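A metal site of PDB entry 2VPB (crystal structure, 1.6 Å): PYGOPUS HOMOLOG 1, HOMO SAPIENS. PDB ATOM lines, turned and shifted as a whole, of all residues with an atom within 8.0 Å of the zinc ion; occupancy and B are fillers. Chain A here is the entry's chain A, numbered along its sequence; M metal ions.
The zinc ion is bound by SG of Cys 27 (2.3 Å), SG of Cys 31 (2.4 Å), SG of Cys 63 (2.4 Å) and SG of Cys 60 (2.4 Å).
Of the 17 residues printed, 4 come within 4 Å of the zinc ion.
The nearest printed residue that does not touch the zinc ion is Ser 30 (4.7 Å).
N of Gln 32 lies within hydrogen-bond range of O of Cys 27, at 3.1 Å.
The side-chain sulfur (SG) of Cys 27 sits close to the backbone NH (N) of Ala 29 (3.5 Å).
N of Cys 27 sits at hydrogen-bond distance from O of Lys 33 (2.9 Å).
The side-chain sulfur (SG) of Cys 31 sits close to the backbone NH (N) of Lys 33, 3.6 Å away.
The backbone NH (N) of Thr 62 lies close to the side-chain sulfur (SG) of Cys 60 (3.6 Å).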
ATOM      1  N   LEU A  26       8.429  14.578  -6.404  1.00  0.00           N
ATOM      2  CA  LEU A  26       9.096  13.313  -6.222  1.00  0.00           C
ATOM      3  C   LEU A  26       8.593  12.333  -7.262  1.00  0.00           C
ATOM      4  O   LEU A  26       7.379  12.192  -7.443  1.00  0.00           O
ATOM      5  CB  LEU A  26       8.773  12.769  -4.816  1.00  0.00           C
ATOM      6  CG  LEU A  26       9.317  11.382  -4.445  1.00  0.00           C
ATOM      7  CD1 LEU A  26      10.830  11.367  -4.338  1.00  0.00           C
ATOM      8  CD2 LEU A  26       8.669  10.905  -3.143  1.00  0.00           C
ATOM      9  N   CYS A  27       9.506  11.630  -7.921  1.00  0.00           N
ATOM     10  CA  CYS A  27       9.070  10.559  -8.810  1.00  0.00           C
ATOM     11  C   CYS A  27       8.618   9.359  -8.001  1.00  0.00           C
ATOM     12  O   CYS A  27       9.405   8.731  -7.289  1.00  0.00           O
ATOM     13  CB  CYS A  27      10.162  10.151  -9.780  1.00  0.00           C
ATOM     14  SG  CYS A  27       9.632   8.725 -10.791  1.00  0.00           S
ATOM     15  N   GLU A  28       7.329   9.048  -8.129  1.00  0.00           N
ATOM     16  CA  GLU A  28       6.761   7.933  -7.386  1.00  0.00           C
ATOM     17  C   GLU A  28       6.394   6.769  -8.308  1.00  0.00           C
ATOM     18  O   GLU A  28       5.624   5.878  -7.930  1.00  0.00           O
ATOM     19  CB  GLU A  28       5.589   8.393  -6.540  1.00  0.00           C
ATOM     20  CG  GLU A  28       6.026   9.347  -5.428  1.00  0.00           C
ATOM     21  CD  GLU A  28       4.890   9.736  -4.504  1.00  0.00           C
ATOM     22  OE1 GLU A  28       4.476   8.883  -3.684  1.00  0.00           O
ATOM     23  OE2 GLU A  28       4.430  10.904  -4.588  1.00  0.00           O
ATOM     24  N   ALA A  29       6.962   6.779  -9.512  1.00  0.00           N
ATOM     25  CA  ALA A  29       6.827   5.650 -10.423  1.00  0.00           C
ATOM     26  C   ALA A  29       7.842   4.576 -10.025  1.00  0.00           C
ATOM     27  O   ALA A  29       7.508   3.393  -9.961  1.00  0.00           O
ATOM     28  CB  ALA A  29       7.022   6.074 -11.867  1.00  0.00           C
ATOM     29  N   SER A  30       9.082   5.001  -9.750  1.00  0.00           N
ATOM     30  CA  SER A  30      10.135   4.060  -9.329  1.00  0.00           C
ATOM     31  C   SER A  30      11.358   4.706  -8.697  1.00  0.00           C
ATOM     32  O   SER A  30      11.761   4.320  -7.595  1.00  0.00           O
ATOM     33  CB  SER A  30      10.599   3.212 -10.508  1.00  0.00           C
ATOM     34  OG  SER A  30      11.625   2.318 -10.100  1.00  0.00           O
ATOM     35  N   CYS A  31      11.960   5.661  -9.402  1.00  0.00           N
ATOM     36  CA  CYS A  31      13.319   6.138  -9.049  1.00  0.00           C
ATOM     37  C   CYS A  31      13.422   6.959  -7.775  1.00  0.00           C
ATOM     38  O   CYS A  31      14.506   7.083  -7.209  1.00  0.00           O
ATOM     39  CB  CYS A  31      13.999   6.860 -10.210  1.00  0.00           C
ATOM     40  SG  CYS A  31      13.408   8.576 -10.525  1.00  0.00           S
ATOM     41  N   GLN A  32      12.312   7.553  -7.334  1.00  0.00           N
ATOM     42  CA  GLN A  32      12.286   8.330  -6.075  1.00  0.00           C
ATOM     43  C   GLN A  32      13.296   9.483  -6.041  1.00  0.00           C
ATOM     44  O   GLN A  32      13.774   9.867  -4.956  1.00  0.00           O
ATOM     45  CB  GLN A  32      12.472   7.399  -4.856  1.00  0.00           C
ATOM     46  CG  GLN A  32      11.298   6.447  -4.621  1.00  0.00           C
ATOM     47  CD  GLN A  32      10.237   7.017  -3.706  1.00  0.00           C
ATOM     48  OE1 GLN A  32       9.187   7.473  -4.161  1.00  0.00           O
ATOM     49  NE2 GLN A  32      10.511   7.000  -2.405  1.00  0.00           N
ATOM     50  N   LYS A  33      13.622  10.033  -7.209  1.00  0.00           N
ATOM     51  CA  LYS A  33      14.388  11.274  -7.282  1.00  0.00           C
ATOM     52  C   LYS A  33      13.451  12.465  -7.103  1.00  0.00           C
ATOM     53  O   LYS A  33      12.276  12.401  -7.480  1.00  0.00           O
ATOM     54  CB  LYS A  33      15.094  11.401  -8.622  1.00  0.00           C
ATOM     55  CG  LYS A  33      16.213  10.421  -8.850  1.00  0.00           C
ATOM     56  CD  LYS A  33      16.803  10.642 -10.228  1.00  0.00           C
ATOM     57  CE  LYS A  33      17.666   9.481 -10.629  1.00  0.00           C
ATOM     58  NZ  LYS A  33      18.141   9.619 -12.025  1.00  0.00           N
ATOM     59  N   TRP A  34      13.974  13.543  -6.537  1.00  0.00           N
ATOM     60  CA  TRP A  34      13.278  14.819  -6.491  1.00  0.00           C
ATOM     61  C   TRP A  34      13.672  15.641  -7.702  1.00  0.00           C
ATOM     62  O   TRP A  34      14.777  15.521  -8.236  1.00  0.00           O
ATOM     63  CB  TRP A  34      13.630  15.586  -5.207  1.00  0.00           C
ATOM     64  CG  TRP A  34      12.975  15.003  -3.977  1.00  0.00           C
ATOM     65  CD1 TRP A  34      13.527  14.096  -3.119  1.00  0.00           C
ATOM     66  CD2 TRP A  34      11.669  15.303  -3.479  1.00  0.00           C
ATOM     67  NE1 TRP A  34      12.636  13.812  -2.110  1.00  0.00           N
ATOM     68  CE2 TRP A  34      11.493  14.535  -2.309  1.00  0.00           C
ATOM     69  CE3 TRP A  34      10.635  16.132  -3.910  1.00  0.00           C
ATOM     70  CZ2 TRP A  34      10.310  14.586  -1.566  1.00  0.00           C
ATOM     71  CZ3 TRP A  34       9.459  16.181  -3.173  1.00  0.00           C
ATOM     72  CH2 TRP A  34       9.309  15.401  -2.016  1.00  0.00           C
ATOM     73  N   PHE A  35      12.738  16.482  -8.143  1.00  0.00           N
ATOM     74  CA  PHE A  35      12.947  17.377  -9.279  1.00  0.00           C
ATOM     75  C   PHE A  35      12.341  18.729  -8.927  1.00  0.00           C
ATOM     76  O   PHE A  35      11.421  18.807  -8.117  1.00  0.00           O
ATOM     77  CB  PHE A  35      12.224  16.860 -10.536  1.00  0.00           C
ATOM     78  CG  PHE A  35      12.625  15.474 -10.995  1.00  0.00           C
ATOM     79  CD1 PHE A  35      13.326  15.313 -12.181  1.00  0.00           C
ATOM     80  CD2 PHE A  35      12.242  14.328 -10.261  1.00  0.00           C
ATOM     81  CE1 PHE A  35      13.684  14.042 -12.644  1.00  0.00           C
ATOM     82  CE2 PHE A  35      12.595  13.051 -10.712  1.00  0.00           C
ATOM     83  CZ  PHE A  35      13.315  12.902 -11.894  1.00  0.00           C
ATOM     84  N   TRP A  58       3.142  11.501  -9.385  1.00  0.00           N
ATOM     85  CA  TRP A  58       3.851  11.816 -10.618  1.00  0.00           C
ATOM     86  C   TRP A  58       4.958  10.801 -10.865  1.00  0.00           C
ATOM     87  O   TRP A  58       5.580  10.285  -9.925  1.00  0.00           O
ATOM     88  CB  TRP A  58       4.454  13.230 -10.508  1.00  0.00           C
ATOM     89  CG  TRP A  58       5.307  13.651 -11.662  1.00  0.00           C
ATOM     90  CD1 TRP A  58       4.891  14.049 -12.909  1.00  0.00           C
ATOM     91  CD2 TRP A  58       6.733  13.711 -11.680  1.00  0.00           C
ATOM     92  NE1 TRP A  58       5.983  14.356 -13.687  1.00  0.00           N
ATOM     93  CE2 TRP A  58       7.129  14.160 -12.958  1.00  0.00           C
ATOM     94  CE3 TRP A  58       7.721  13.439 -10.721  1.00  0.00           C
ATOM     95  CZ2 TRP A  58       8.478  14.340 -13.303  1.00  0.00           C
ATOM     96  CZ3 TRP A  58       9.052  13.608 -11.070  1.00  0.00           C
ATOM     97  CH2 TRP A  58       9.424  14.061 -12.345  1.00  0.00           C
ATOM     98  N   GLY A  59       5.210  10.553 -12.149  1.00  0.00           N
ATOM     99  CA  GLY A  59       6.337   9.735 -12.570  1.00  0.00           C
ATOM    100  C   GLY A  59       7.154  10.505 -13.584  1.00  0.00           C
ATOM    101  O   GLY A  59       6.613  11.140 -14.493  1.00  0.00           O
ATOM    102  N   CYS A  60       8.477  10.414 -13.459  1.00  0.00           N
ATOM    103  CA  CYS A  60       9.362  11.109 -14.386  1.00  0.00           C
ATOM    104  C   CYS A  60       9.349  10.457 -15.773  1.00  0.00           C
ATOM    105  O   CYS A  60       8.908   9.329 -15.930  1.00  0.00           O
ATOM    106  CB  CYS A  60      10.783  11.220 -13.826  1.00  0.00           C
ATOM    107  SG  CYS A  60      11.760   9.675 -13.954  1.00  0.00           S
ATOM    108  N   ASP A  61       9.832  11.189 -16.777  1.00  0.00           N
ATOM    109  CA  ASP A  61       9.822  10.719 -18.149  1.00  0.00           C
ATOM    110  C   ASP A  61      10.584   9.403 -18.279  1.00  0.00           C
ATOM    111  O   ASP A  61      10.167   8.514 -19.026  1.00  0.00           O
ATOM    112  CB  ASP A  61      10.411  11.777 -19.087  1.00  0.00           C
ATOM    113  CG  ASP A  61       9.529  13.034 -19.191  1.00  0.00           C
ATOM    114  OD1 ASP A  61       8.375  13.020 -18.725  1.00  0.00           O
ATOM    115  OD2 ASP A  61       9.998  14.035 -19.783  1.00  0.00           O
ATOM    116  N   THR A  62      11.666   9.262 -17.531  1.00  0.00           N
ATOM    117  CA  THR A  62      12.476   8.036 -17.614  1.00  0.00           C
ATOM    118  C   THR A  62      11.738   6.801 -17.085  1.00  0.00           C
ATOM    119  O   THR A  62      11.711   5.749 -17.733  1.00  0.00           O
ATOM    120  CB  THR A  62      13.822   8.195 -16.905  1.00  0.00           C
ATOM    121  OG1 THR A  62      14.500   9.346 -17.434  1.00  0.00           O
ATOM    122  CG2 THR A  62      14.696   6.961 -17.116  1.00  0.00           C
ATOM    123  N   CYS A  63      11.130   6.932 -15.906  1.00  0.00           N
ATOM    124  CA  CYS A  63      10.414   5.822 -15.307  1.00  0.00           C
ATOM    125  C   CYS A  63       9.114   5.508 -16.061  1.00  0.00           C
ATOM    126  O   CYS A  63       8.673   4.364 -16.072  1.00  0.00           O
ATOM    127  CB  CYS A  63      10.118   6.107 -13.836  1.00  0.00           C
ATOM    128  SG  CYS A  63      11.550   6.124 -12.764  1.00  0.00           S
ATOM    129  N   MET A  64       8.512   6.524 -16.679  1.00  0.00           N
ATOM    130  CA  MET A  64       7.268   6.334 -17.400  1.00  0.00           C
ATOM    131  C   MET A  64       7.486   5.751 -18.802  1.00  0.00           C
ATOM    132  O   MET A  64       6.593   5.102 -19.342  1.00  0.00           O
ATOM    133  CB  MET A  64       6.465   7.643 -17.504  1.00  0.00           C
ATOM    134  CG  MET A  64       5.965   8.186 -16.173  1.00  0.00           C
ATOM    135  SD  MET A  64       4.957   7.031 -15.230  1.00  0.00           S
ATOM    136  CE  MET A  64       3.388   7.164 -16.079  1.00  0.00           C
HETATM  137 ZN    ZN M   1      11.580   8.352 -11.987  1.00  0.00          ZN
